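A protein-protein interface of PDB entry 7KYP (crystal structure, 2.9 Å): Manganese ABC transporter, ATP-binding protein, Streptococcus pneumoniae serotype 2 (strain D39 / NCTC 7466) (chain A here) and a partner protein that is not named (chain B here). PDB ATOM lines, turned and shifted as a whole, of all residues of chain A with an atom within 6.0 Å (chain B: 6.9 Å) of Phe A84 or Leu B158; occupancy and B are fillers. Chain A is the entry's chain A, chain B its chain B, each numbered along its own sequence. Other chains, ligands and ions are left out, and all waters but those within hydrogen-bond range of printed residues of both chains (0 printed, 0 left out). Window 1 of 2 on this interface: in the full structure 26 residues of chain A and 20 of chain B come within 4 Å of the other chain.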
ATOM      1  N   ASP A  81      33.842   3.672 -21.004  1.00  0.00           N
ATOM      2  CA  ASP A  81      34.789   3.312 -19.950  1.00  0.00           C
ATOM      3  C   ASP A  81      34.673   1.823 -19.638  1.00  0.00           C
ATOM      4  O   ASP A  81      33.659   1.373 -19.104  1.00  0.00           O
ATOM      5  CB  ASP A  81      34.519   4.141 -18.689  1.00  0.00           C
ATOM      6  CG  ASP A  81      35.492   3.837 -17.558  1.00  0.00           C
ATOM      7  OD1 ASP A  81      36.670   3.525 -17.835  1.00  0.00           O
ATOM      8  OD2 ASP A  81      35.077   3.923 -16.384  1.00  0.00           O
ATOM      9  N   TYR A  82      35.722   1.069 -19.964  1.00  0.00           N
ATOM     10  CA  TYR A  82      35.721  -0.389 -19.790  1.00  0.00           C
ATOM     11  C   TYR A  82      35.761  -0.782 -18.313  1.00  0.00           C
ATOM     12  O   TYR A  82      35.256  -1.839 -17.933  1.00  0.00           O
ATOM     13  CB  TYR A  82      36.912  -1.028 -20.512  1.00  0.00           C
ATOM     14  CG  TYR A  82      37.077  -0.611 -21.959  1.00  0.00           C
ATOM     15  CD1 TYR A  82      36.222  -1.094 -22.946  1.00  0.00           C
ATOM     16  CD2 TYR A  82      38.094   0.260 -22.341  1.00  0.00           C
ATOM     17  CE1 TYR A  82      36.371  -0.715 -24.270  1.00  0.00           C
ATOM     18  CE2 TYR A  82      38.251   0.643 -23.661  1.00  0.00           C
ATOM     19  CZ  TYR A  82      37.388   0.154 -24.622  1.00  0.00           C
ATOM     20  OH  TYR A  82      37.546   0.534 -25.935  1.00  0.00           O
ATOM     21  N   ASN A  83      36.359   0.076 -17.490  1.00  0.00           N
ATOM     22  CA  ASN A  83      36.525  -0.195 -16.063  1.00  0.00           C
ATOM     23  C   ASN A  83      35.254   0.024 -15.234  1.00  0.00           C
ATOM     24  O   ASN A  83      35.224  -0.324 -14.053  1.00  0.00           O
ATOM     25  CB  ASN A  83      37.653   0.670 -15.498  1.00  0.00           C
ATOM     26  CG  ASN A  83      38.999   0.374 -16.136  1.00  0.00           C
ATOM     27  OD1 ASN A  83      39.284  -0.761 -16.521  1.00  0.00           O
ATOM     28  ND2 ASN A  83      39.839   1.396 -16.242  1.00  0.00           N
ATOM     29  N   PHE A  84      34.220   0.605 -15.841  1.00  0.00           N
ATOM     30  CA  PHE A  84      32.936   0.812 -15.167  1.00  0.00           C
ATOM     31  C   PHE A  84      32.363  -0.525 -14.684  1.00  0.00           C
ATOM     32  O   PHE A  84      32.414  -1.514 -15.418  1.00  0.00           O
ATOM     33  CB  PHE A  84      31.942   1.493 -16.118  1.00  0.00           C
ATOM     34  CG  PHE A  84      30.727   2.051 -15.433  1.00  0.00           C
ATOM     35  CD1 PHE A  84      29.616   1.252 -15.192  1.00  0.00           C
ATOM     36  CD2 PHE A  84      30.690   3.380 -15.032  1.00  0.00           C
ATOM     37  CE1 PHE A  84      28.496   1.765 -14.559  1.00  0.00           C
ATOM     38  CE2 PHE A  84      29.571   3.900 -14.400  1.00  0.00           C
ATOM     39  CZ  PHE A  84      28.473   3.091 -14.163  1.00  0.00           C
ATOM     40  N   PRO A  85      31.820  -0.562 -13.451  1.00  0.00           N
ATOM     41  CA  PRO A  85      31.263  -1.813 -12.936  1.00  0.00           C
ATOM     42  C   PRO A  85      29.910  -2.142 -13.569  1.00  0.00           C
ATOM     43  O   PRO A  85      28.883  -1.585 -13.176  1.00  0.00           O
ATOM     44  CB  PRO A  85      31.121  -1.542 -11.434  1.00  0.00           C
ATOM     45  CG  PRO A  85      30.919  -0.072 -11.339  1.00  0.00           C
ATOM     46  CD  PRO A  85      31.688   0.539 -12.477  1.00  0.00           C
ATOM     47  N   ILE A  86      29.926  -3.036 -14.553  1.00  0.00           N
ATOM     48  CA  ILE A  86      28.714  -3.433 -15.264  1.00  0.00           C
ATOM     49  C   ILE A  86      28.956  -4.734 -16.033  1.00  0.00           C
ATOM     50  O   ILE A  86      29.967  -4.874 -16.727  1.00  0.00           O
ATOM     51  CB  ILE A  86      28.227  -2.313 -16.222  1.00  0.00           C
ATOM     52  CG1 ILE A  86      26.876  -2.678 -16.847  1.00  0.00           C
ATOM     53  CG2 ILE A  86      29.262  -2.017 -17.303  1.00  0.00           C
ATOM     54  CD1 ILE A  86      26.225  -1.534 -17.596  1.00  0.00           C
ATOM     55  N   GLU A  90      23.910  -6.722 -18.327  1.00  0.00           N
ATOM     56  CA  GLU A  90      23.476  -5.436 -17.790  1.00  0.00           C
ATOM     57  C   GLU A  90      23.774  -4.297 -18.766  1.00  0.00           C
ATOM     58  O   GLU A  90      23.030  -3.317 -18.827  1.00  0.00           O
ATOM     59  CB  GLU A  90      24.148  -5.176 -16.439  1.00  0.00           C
ATOM     60  CG  GLU A  90      23.543  -4.024 -15.648  1.00  0.00           C
ATOM     61  CD  GLU A  90      23.927  -4.049 -14.178  1.00  0.00           C
ATOM     62  OE1 GLU A  90      24.944  -4.687 -13.826  1.00  0.00           O
ATOM     63  OE2 GLU A  90      23.208  -3.425 -13.368  1.00  0.00           O
ATOM     64  N   LEU A  94      20.659  -1.960 -21.265  1.00  0.00           N
ATOM     65  CA  LEU A  94      20.540  -0.496 -21.315  1.00  0.00           C
ATOM     66  C   LEU A  94      19.729   0.000 -22.516  1.00  0.00           C
ATOM     67  O   LEU A  94      19.098   1.055 -22.444  1.00  0.00           O
ATOM     68  CB  LEU A  94      21.924   0.162 -21.343  1.00  0.00           C
ATOM     69  CG  LEU A  94      22.895  -0.129 -20.194  1.00  0.00           C
ATOM     70  CD1 LEU A  94      24.146   0.720 -20.358  1.00  0.00           C
ATOM     71  CD2 LEU A  94      22.251   0.107 -18.834  1.00  0.00           C
ATOM     72  N   PHE A  97      15.964   0.516 -21.748  1.00  0.00           N
ATOM     73  CA  PHE A  97      15.597   1.518 -20.734  1.00  0.00           C
ATOM     74  C   PHE A  97      14.617   2.596 -21.227  1.00  0.00           C
ATOM     75  O   PHE A  97      13.741   3.013 -20.467  1.00  0.00           O
ATOM     76  CB  PHE A  97      16.859   2.172 -20.139  1.00  0.00           C
ATOM     77  CG  PHE A  97      17.577   1.323 -19.112  1.00  0.00           C
ATOM     78  CD1 PHE A  97      17.501  -0.070 -19.130  1.00  0.00           C
ATOM     79  CD2 PHE A  97      18.361   1.926 -18.137  1.00  0.00           C
ATOM     80  CE1 PHE A  97      18.173  -0.831 -18.189  1.00  0.00           C
ATOM     81  CE2 PHE A  97      19.038   1.167 -17.196  1.00  0.00           C
ATOM     82  CZ  PHE A  97      18.943  -0.214 -17.220  1.00  0.00           C
ATOM     83  N   GLN A 130      32.423  -9.344 -16.573  1.00  0.00           N
ATOM     84  CA  GLN A 130      32.737  -7.920 -16.683  1.00  0.00           C
ATOM     85  C   GLN A 130      33.103  -7.549 -18.116  1.00  0.00           C
ATOM     86  O   GLN A 130      33.747  -8.330 -18.818  1.00  0.00           O
ATOM     87  CB  GLN A 130      33.899  -7.552 -15.754  1.00  0.00           C
ATOM     88  CG  GLN A 130      33.581  -7.676 -14.273  1.00  0.00           C
ATOM     89  CD  GLN A 130      32.698  -6.551 -13.775  1.00  0.00           C
ATOM     90  OE1 GLN A 130      31.511  -6.746 -13.525  1.00  0.00           O
ATOM     91  NE2 GLN A 130      33.273  -5.361 -13.642  1.00  0.00           N
ATOM     92  N   ILE A 131      32.701  -6.354 -18.539  1.00  0.00           N
ATOM     93  CA  ILE A 131      33.058  -5.844 -19.869  1.00  0.00           C
ATOM     94  C   ILE A 131      34.561  -5.574 -20.001  1.00  0.00           C
ATOM     95  O   ILE A 131      35.097  -5.565 -21.110  1.00  0.00           O
ATOM     96  CB  ILE A 131      32.256  -4.575 -20.252  1.00  0.00           C
ATOM     97  CG1 ILE A 131      32.534  -3.415 -19.287  1.00  0.00           C
ATOM     98  CG2 ILE A 131      30.766  -4.885 -20.300  1.00  0.00           C
ATOM     99  CD1 ILE A 131      31.929  -2.099 -19.728  1.00  0.00           C
ATOM    100  N   SER A 132      35.232  -5.352 -18.872  1.00  0.00           N
ATOM    101  CA  SER A 132      36.691  -5.234 -18.837  1.00  0.00           C
ATOM    102  C   SER A 132      37.380  -6.562 -19.165  1.00  0.00           C
ATOM    103  O   SER A 132      38.488  -6.573 -19.702  1.00  0.00           O
ATOM    104  CB  SER A 132      37.153  -4.743 -17.463  1.00  0.00           C
ATOM    105  OG  SER A 132      36.625  -5.553 -16.426  1.00  0.00           O
ATOM    106  N   CYS B  34      29.626   7.076  -4.989  1.00  0.00           N
ATOM    107  CA  CYS B  34      29.806   6.183  -6.137  1.00  0.00           C
ATOM    108  C   CYS B  34      29.604   6.915  -7.460  1.00  0.00           C
ATOM    109  O   CYS B  34      30.397   6.761  -8.385  1.00  0.00           O
ATOM    110  CB  CYS B  34      28.843   4.995  -6.057  1.00  0.00           C
ATOM    111  SG  CYS B  34      29.299   3.772  -4.811  1.00  0.00           S
ATOM    112  N   PHE B  35      28.541   7.712  -7.537  1.00  0.00           N
ATOM    113  CA  PHE B  35      28.233   8.479  -8.742  1.00  0.00           C
ATOM    114  C   PHE B  35      29.211   9.636  -8.953  1.00  0.00           C
ATOM    115  O   PHE B  35      29.480  10.023 -10.089  1.00  0.00           O
ATOM    116  CB  PHE B  35      26.798   9.008  -8.687  1.00  0.00           C
ATOM    117  CG  PHE B  35      25.757   7.926  -8.647  1.00  0.00           C
ATOM    118  CD1 PHE B  35      25.392   7.256  -9.806  1.00  0.00           C
ATOM    119  CD2 PHE B  35      25.147   7.571  -7.451  1.00  0.00           C
ATOM    120  CE1 PHE B  35      24.436   6.253  -9.773  1.00  0.00           C
ATOM    121  CE2 PHE B  35      24.191   6.570  -7.413  1.00  0.00           C
ATOM    122  CZ  PHE B  35      23.834   5.911  -8.577  1.00  0.00           C
ATOM    123  N   LEU B  38      32.577   7.987 -10.383  1.00  0.00           N
ATOM    124  CA  LEU B  38      32.321   7.349 -11.679  1.00  0.00           C
ATOM    125  C   LEU B  38      32.091   8.379 -12.788  1.00  0.00           C
ATOM    126  O   LEU B  38      32.499   8.165 -13.931  1.00  0.00           O
ATOM    127  CB  LEU B  38      31.122   6.396 -11.598  1.00  0.00           C
ATOM    128  CG  LEU B  38      31.341   5.072 -10.862  1.00  0.00           C
ATOM    129  CD1 LEU B  38      30.009   4.358 -10.688  1.00  0.00           C
ATOM    130  CD2 LEU B  38      32.343   4.187 -11.589  1.00  0.00           C
ATOM    131  N   ARG B  39      31.440   9.489 -12.445  1.00  0.00           N
ATOM    132  CA  ARG B  39      31.167  10.562 -13.406  1.00  0.00           C
ATOM    133  C   ARG B  39      32.310  11.582 -13.496  1.00  0.00           C
ATOM    134  O   ARG B  39      32.250  12.508 -14.306  1.00  0.00           O
ATOM    135  CB  ARG B  39      29.859  11.272 -13.048  1.00  0.00           C
ATOM    136  CG  ARG B  39      28.636  10.365 -13.090  1.00  0.00           C
ATOM    137  CD  ARG B  39      27.445  10.987 -12.379  1.00  0.00           C
ATOM    138  NE  ARG B  39      26.766  11.993 -13.196  1.00  0.00           N
ATOM    139  CZ  ARG B  39      25.741  11.757 -14.018  1.00  0.00           C
ATOM    140  NH1 ARG B  39      25.240  10.533 -14.166  1.00  0.00           N
ATOM    141  NH2 ARG B  39      25.210  12.763 -14.704  1.00  0.00           N
ATOM    142  N   PHE B 153      15.546   6.625  -9.506  1.00  0.00           N
ATOM    143  CA  PHE B 153      16.273   6.981 -10.728  1.00  0.00           C
ATOM    144  C   PHE B 153      17.559   6.165 -10.919  1.00  0.00           C
ATOM    145  O   PHE B 153      18.535   6.669 -11.478  1.00  0.00           O
ATOM    146  CB  PHE B 153      16.611   8.478 -10.724  1.00  0.00           C
ATOM    147  CG  PHE B 153      15.405   9.377 -10.716  1.00  0.00           C
ATOM    148  CD1 PHE B 153      14.543   9.415 -11.805  1.00  0.00           C
ATOM    149  CD2 PHE B 153      15.140  10.203  -9.629  1.00  0.00           C
ATOM    150  CE1 PHE B 153      13.434  10.245 -11.805  1.00  0.00           C
ATOM    151  CE2 PHE B 153      14.034  11.036  -9.624  1.00  0.00           C
ATOM    152  CZ  PHE B 153      13.179  11.058 -10.714  1.00  0.00           C
ATOM    153  N   PHE B 154      17.558   4.907 -10.479  1.00  0.00           N
ATOM    154  CA  PHE B 154      18.750   4.059 -10.569  1.00  0.00           C
ATOM    155  C   PHE B 154      19.112   3.736 -12.018  1.00  0.00           C
ATOM    156  O   PHE B 154      20.279   3.801 -12.401  1.00  0.00           O
ATOM    157  CB  PHE B 154      18.549   2.758  -9.784  1.00  0.00           C
ATOM    158  CG  PHE B 154      19.764   1.872  -9.756  1.00  0.00           C
ATOM    159  CD1 PHE B 154      20.810   2.136  -8.880  1.00  0.00           C
ATOM    160  CD2 PHE B 154      19.864   0.776 -10.601  1.00  0.00           C
ATOM    161  CE1 PHE B 154      21.931   1.322  -8.850  1.00  0.00           C
ATOM    162  CE2 PHE B 154      20.982  -0.041 -10.576  1.00  0.00           C
ATOM    163  CZ  PHE B 154      22.017   0.232  -9.699  1.00  0.00           C
ATOM    164  N   LYS B 155      18.105   3.381 -12.812  1.00  0.00           N
ATOM    165  CA  LYS B 155      18.304   3.063 -14.227  1.00  0.00           C
ATOM    166  C   LYS B 155      18.737   4.284 -15.040  1.00  0.00           C
ATOM    167  O   LYS B 155      19.532   4.165 -15.973  1.00  0.00           O
ATOM    168  CB  LYS B 155      17.031   2.456 -14.830  1.00  0.00           C
ATOM    169  CG  LYS B 155      16.851   0.977 -14.521  1.00  0.00           C
ATOM    170  CD  LYS B 155      15.753   0.342 -15.365  1.00  0.00           C
ATOM    171  CE  LYS B 155      14.362   0.826 -14.977  1.00  0.00           C
ATOM    172  NZ  LYS B 155      13.998   0.466 -13.579  1.00  0.00           N
ATOM    173  N   GLN B 156      18.219   5.453 -14.675  1.00  0.00           N
ATOM    174  CA  GLN B 156      18.541   6.694 -15.382  1.00  0.00           C
ATOM    175  C   GLN B 156      19.941   7.189 -15.015  1.00  0.00           C
ATOM    176  O   GLN B 156      20.665   7.702 -15.868  1.00  0.00           O
ATOM    177  CB  GLN B 156      17.495   7.778 -15.089  1.00  0.00           C
ATOM    178  CG  GLN B 156      16.173   7.586 -15.824  1.00  0.00           C
ATOM    179  CD  GLN B 156      15.355   6.417 -15.304  1.00  0.00           C
ATOM    180  OE1 GLN B 156      15.249   6.205 -14.096  1.00  0.00           O
ATOM    181  NE2 GLN B 156      14.764   5.658 -16.218  1.00  0.00           N
ATOM    182  N   LEU B 157      20.311   7.032 -13.746  1.00  0.00           N
ATOM    183  CA  LEU B 157      21.650   7.389 -13.274  1.00  0.00           C
ATOM    184  C   LEU B 157      22.719   6.414 -13.774  1.00  0.00           C
ATOM    185  O   LEU B 157      23.890   6.780 -13.890  1.00  0.00           O
ATOM    186  CB  LEU B 157      21.682   7.457 -11.744  1.00  0.00           C
ATOM    187  CG  LEU B 157      20.951   8.649 -11.114  1.00  0.00           C
ATOM    188  CD1 LEU B 157      20.671   8.395  -9.639  1.00  0.00           C
ATOM    189  CD2 LEU B 157      21.745   9.935 -11.298  1.00  0.00           C
ATOM    190  N   LEU B 158      22.314   5.179 -14.063  1.00  0.00           N
ATOM    191  CA  LEU B 158      23.230   4.153 -14.566  1.00  0.00           C
ATOM    192  C   LEU B 158      23.745   4.486 -15.967  1.00  0.00           C
ATOM    193  O   LEU B 158      24.957   4.531 -16.187  1.00  0.00           O
ATOM    194  CB  LEU B 158      22.548   2.778 -14.563  1.00  0.00           C
ATOM    195  CG  LEU B 158      23.321   1.581 -15.129  1.00  0.00           C
ATOM    196  CD1 LEU B 158      24.722   1.477 -14.546  1.00  0.00           C
ATOM    197  CD2 LEU B 158      22.543   0.297 -14.878  1.00  0.00           C
ATOM    198  N   ILE B 159      22.827   4.722 -16.904  1.00  0.00           N
ATOM    199  CA  ILE B 159      23.198   5.016 -18.294  1.00  0.00           C
ATOM    200  C   ILE B 159      23.969   6.329 -18.401  1.00  0.00           C
ATOM    201  O   ILE B 159      24.986   6.394 -19.087  1.00  0.00           O
ATOM    202  CB  ILE B 159      21.971   5.063 -19.237  1.00  0.00           C
ATOM    203  CG1 ILE B 159      21.336   3.672 -19.342  1.00  0.00           C
ATOM    204  CG2 ILE B 159      22.372   5.547 -20.631  1.00  0.00           C
ATOM    205  CD1 ILE B 159      20.227   3.560 -20.369  1.00  0.00           C
ATOM    206  N   THR B 160      23.487   7.367 -17.721  1.00  0.00           N
ATOM    207  CA  THR B 160      24.100   8.694 -17.801  1.00  0.00           C
ATOM    208  C   THR B 160      25.526   8.720 -17.243  1.00  0.00           C
ATOM    209  O   THR B 160      26.372   9.466 -17.736  1.00  0.00           O
ATOM    210  CB  THR B 160      23.249   9.753 -17.071  1.00  0.00           C
ATOM    211  OG1 THR B 160      22.988   9.324 -15.730  1.00  0.00           O
ATOM    212  CG2 THR B 160      21.928   9.978 -17.804  1.00  0.00           C
ATOM    213  N   SER B 161      25.787   7.906 -16.222  1.00  0.00           N
ATOM    214  CA  SER B 161      27.126   7.790 -15.640  1.00  0.00           C
ATOM    215  C   SER B 161      28.060   6.930 -16.496  1.00  0.00           C
ATOM    216  O   SER B 161      29.241   7.244 -16.644  1.00  0.00           O
ATOM    217  CB  SER B 161      27.042   7.205 -14.228  1.00  0.00           C
ATOM    218  OG  SER B 161      26.248   8.021 -13.384  1.00  0.00           O
ATOM    219  N   PHE B 162      27.522   5.846 -17.053  1.00  0.00           N
ATOM    220  CA  PHE B 162      28.307   4.895 -17.847  1.00  0.00           C
ATOM    221  C   PHE B 162      28.508   5.371 -19.285  1.00  0.00           C
ATOM    222  O   PHE B 162      29.632   5.392 -19.789  1.00  0.00           O
ATOM    223  CB  PHE B 162      27.628   3.520 -17.835  1.00  0.00           C
ATOM    224  CG  PHE B 162      28.239   2.522 -18.782  1.00  0.00           C
ATOM    225  CD1 PHE B 162      29.590   2.206 -18.707  1.00  0.00           C
ATOM    226  CD2 PHE B 162      27.461   1.887 -19.740  1.00  0.00           C
ATOM    227  CE1 PHE B 162      30.151   1.285 -19.577  1.00  0.00           C
ATOM    228  CE2 PHE B 162      28.016   0.965 -20.612  1.00  0.00           C
ATOM    229  CZ  PHE B 162      29.364   0.663 -20.530  1.00  0.00           C
ATOM    230  N   ASP B 163      27.410   5.741 -19.938  1.00  0.00           N
ATOM    231  CA  ASP B 163      27.424   6.112 -21.351  1.00  0.00           C
ATOM    232  C   ASP B 163      26.467   7.281 -21.593  1.00  0.00           C
ATOM    233  O   ASP B 163      25.302   7.088 -21.943  1.00  0.00           O
ATOM    234  CB  ASP B 163      27.041   4.894 -22.203  1.00  0.00           C
ATOM    235  CG  ASP B 163      27.313   5.096 -23.684  1.00  0.00           C
ATOM    236  OD1 ASP B 163      27.361   6.258 -24.140  1.00  0.00           O
ATOM    237  OD2 ASP B 163      27.470   4.085 -24.398  1.00  0.00           O
ATOM    238  N   GLU B 164      26.974   8.496 -21.402  1.00  0.00           N
ATOM    239  CA  GLU B 164      26.174   9.708 -21.580  1.00  0.00           C
ATOM    240  C   GLU B 164      25.850   9.965 -23.054  1.00  0.00           C
ATOM    241  O   GLU B 164      24.827  10.573 -23.370  1.00  0.00           O
ATOM    242  CB  GLU B 164      26.897  10.923 -20.990  1.00  0.00           C
ATOM    243  CG  GLU B 164      25.982  12.108 -20.713  1.00  0.00           C
ATOM    244  CD  GLU B 164      26.743  13.361 -20.329  1.00  0.00           C
ATOM    245  OE1 GLU B 164      27.618  13.791 -21.109  1.00  0.00           O
ATOM    246  OE2 GLU B 164      26.454  13.924 -19.251  1.00  0.00           O
ATOM    247  N   TYR B 213      35.046   0.527  -5.533  1.00  0.00           N
ATOM    248  CA  TYR B 213      35.339   0.474  -6.966  1.00  0.00           C
ATOM    249  C   TYR B 213      36.359  -0.622  -7.301  1.00  0.00           C
ATOM    250  O   TYR B 213      36.338  -1.179  -8.399  1.00  0.00           O
ATOM    251  CB  TYR B 213      35.842   1.850  -7.429  1.00  0.00           C
ATOM    252  CG  TYR B 213      35.937   2.076  -8.927  1.00  0.00           C
ATOM    253  CD1 TYR B 213      35.137   1.374  -9.831  1.00  0.00           C
ATOM    254  CD2 TYR B 213      36.802   3.039  -9.436  1.00  0.00           C
ATOM    255  CE1 TYR B 213      35.228   1.606 -11.194  1.00  0.00           C
ATOM    256  CE2 TYR B 213      36.894   3.278 -10.794  1.00  0.00           C
ATOM    257  CZ  TYR B 213      36.108   2.559 -11.669  1.00  0.00           C
ATOM    258  OH  TYR B 213      36.201   2.796 -13.022  1.00  0.00           O
ATOM    259  N   ALA B 216      33.767  -4.068  -6.652  1.00  0.00           N
ATOM    260  CA  ALA B 216      32.416  -4.243  -7.196  1.00  0.00           C
ATOM    261  C   ALA B 216      32.360  -4.676  -8.659  1.00  0.00           C
ATOM    262  O   ALA B 216      33.178  -4.254  -9.477  1.00  0.00           O
ATOM    263  CB  ALA B 216      31.614  -2.963  -7.008  1.00  0.00           C
ATOM    264  N   ASN B 217      31.375  -5.521  -8.965  1.00  0.00           N
ATOM    265  CA  ASN B 217      31.103  -5.988 -10.327  1.00  0.00           C
ATOM    266  C   ASN B 217      29.797  -5.401 -10.879  1.00  0.00           C
ATOM    267  O   ASN B 217      29.339  -5.798 -11.953  1.00  0.00           O
ATOM    268  CB  ASN B 217      31.029  -7.517 -10.346  1.00  0.00           C
ATOM    269  CG  ASN B 217      32.340  -8.172  -9.954  1.00  0.00           C
ATOM    270  OD1 ASN B 217      33.415  -7.744 -10.377  1.00  0.00           O
ATOM    271  ND2 ASN B 217      32.257  -9.222  -9.144  1.00  0.00           N
ATOM    272  N   SER B 218      29.197  -4.465 -10.145  1.00  0.00           N
ATOM    273  CA  SER B 218      27.985  -3.779 -10.593  1.00  0.00           C
ATOM    274  C   SER B 218      27.757  -2.514  -9.771  1.00  0.00           C
ATOM    275  O   SER B 218      28.284  -2.379  -8.664  1.00  0.00           O
ATOM    276  CB  SER B 218      26.764  -4.699 -10.486  1.00  0.00           C
ATOM    277  OG  SER B 218      26.529  -5.094  -9.146  1.00  0.00           O
ATOM    278  N   LEU B 219      26.965  -1.596 -10.318  1.00  0.00           N
ATOM    279  CA  LEU B 219      26.657  -0.335  -9.646  1.00  0.00           C
ATOM    280  C   LEU B 219      25.937  -0.574  -8.318  1.00  0.00           C
ATOM    281  O   LEU B 219      26.229   0.090  -7.323  1.00  0.00           O
ATOM    282  CB  LEU B 219      25.810   0.564 -10.553  1.00  0.00           C
ATOM    283  CG  LEU B 219      25.575   2.002 -10.078  1.00  0.00           C
ATOM    284  CD1 LEU B 219      26.888   2.766  -9.971  1.00  0.00           C
ATOM    285  CD2 LEU B 219      24.612   2.725 -11.009  1.00  0.00           C
ATOM    286  N   MET B 222      28.463  -1.908  -5.957  1.00  0.00           N
ATOM    287  CA  MET B 222      29.383  -0.834  -5.579  1.00  0.00           C
ATOM    288  C   MET B 222      28.787   0.078  -4.506  1.00  0.00           C
ATOM    289  O   MET B 222      29.483   0.458  -3.563  1.00  0.00           O
ATOM    290  CB  MET B 222      29.773  -0.010  -6.810  1.00  0.00           C
ATOM    291  CG  MET B 222      30.952   0.924  -6.589  1.00  0.00           C
ATOM    292  SD  MET B 222      31.295   1.951  -8.029  1.00  0.00           S
ATOM    293  CE  MET B 222      32.477   3.110  -7.351  1.00  0.00           C
ATOM    294  N   LYS B 269      40.827  -7.560  -8.428  1.00  0.00           N
ATOM    295  CA  LYS B 269      41.151  -6.728  -9.591  1.00  0.00           C
ATOM    296  C   LYS B 269      42.517  -6.051  -9.443  1.00  0.00           C
ATOM    297  O   LYS B 269      43.221  -5.851 -10.434  1.00  0.00           O
ATOM    298  CB  LYS B 269      40.062  -5.678  -9.836  1.00  0.00           C
ATOM    299  CG  LYS B 269      38.732  -6.267 -10.288  1.00  0.00           C
ATOM    300  CD  LYS B 269      37.809  -5.216 -10.892  1.00  0.00           C
ATOM    301  CE  LYS B 269      37.306  -4.232  -9.847  1.00  0.00           C
ATOM    302  NZ  LYS B 269      36.325  -3.260 -10.405  1.00  0.00           N
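The backbone NH (N) of Leu B219 is in hydrogen-bond range of the backbone carbonyl oxygen (O) of Pro A85 (3.4 Å).
The backbone carbonyl oxygen (O) of Asn B217 sits close to the side-chain amide oxygen (OE1) of Gln A130, at 2.8 Å.
O of Asn A83 is in hydrogen-bond range of OH of Tyr B213.
The backbone carbonyl oxygen (O) of Met B222 sits at hydrogen-bond distance from the side-chain sulfur (SG) of Cys B34, 3.5 Å away.
The side-chain hydroxyl of Ser B161 sits at hydrogen-bond distance from the guanidinium group of Arg B39.
O of Ala B216 lies within hydrogen-bond range of NZ of Lys B269 (3.4 Å).
The side-chain amino group (NZ) of Lys B269 is in hydrogen-bond range of the backbone carbonyl oxygen (O) of Tyr B213, at 2.9 Å.
OD1 of Asp A81 sits close to N of Asn A83 (3.5 Å).
The side-chain carboxylate (OD2) of Asp A81 lies within hydrogen-bond range of the backbone NH (N) of Phe A84, 3.5 Å away.
Among the printed residues, merely in contact across the chains: Asp A81 with Phe B162 (3.5 Å), Asp A81 with Tyr B213 (3.7 Å), Phe A84 with Leu B38 (3.8 Å), Phe A84 with Leu B158 (3.8 Å), Phe A84 with Ser B161 (3.98 Å), Phe A84 with Phe B162 (3.5 Å), Pro A85 with Leu B38 (3.8 Å), Pro A85 with Tyr B213 (3.9 Å), Pro A85 with Ala B216 (3.9 Å), Pro A85 with Ser B218 (3.5 Å), Pro A85 with Met B222 (3.9 Å), Ile A86 with Asn B217 (3.8 Å), Glu A90 with Ser B218 (3.8 Å), Leu A94 with Leu B158 (3.97 Å), Leu A94 with Ile B159 (3.4 Å), Leu A94 with Phe B162 (3.6 Å), Phe A97 with Lys B155 (3.3 Å), Phe A97 with Ile B159 (3.3 Å) and Ile A131 with Phe B162 (3.8 Å).
Of the printed residues of chain B, Phe A84 touches Leu B38, Leu B158, Ser B161 and Phe B162.
Leu B158 touches two residues of chain A.
Of the printed residues of chain A, Phe B162 touches Asp A81, Phe A84, Leu A94 and Ile A131.
Asp B163 touches none of the printed residues of chain A.
Printed residues of chain A within 4 Å of Tyr B213: Asp A81, Asn A83 and Pro A85.
Of the printed residues of chain A, Ser B218 touches Pro A85 and Glu A90.
The nearest printed residue of chain B that does not touch Phe A84 is Tyr B213 (4.1 Å).
The nearest printed residue of chain A that does not touch Lys B155 is Leu A94 (5.7 Å).
Along chain B the printed residues that touch a printed residue of chain A span positions 38 to 222.
Hydrophobic or aromatic side chains of chain A within 4 Å of the printed part of chain B: Phe A84, Pro A85, Leu A94, Phe A97 and Ile A131.
Among the printed residues, 22 pairs touch across the chains.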
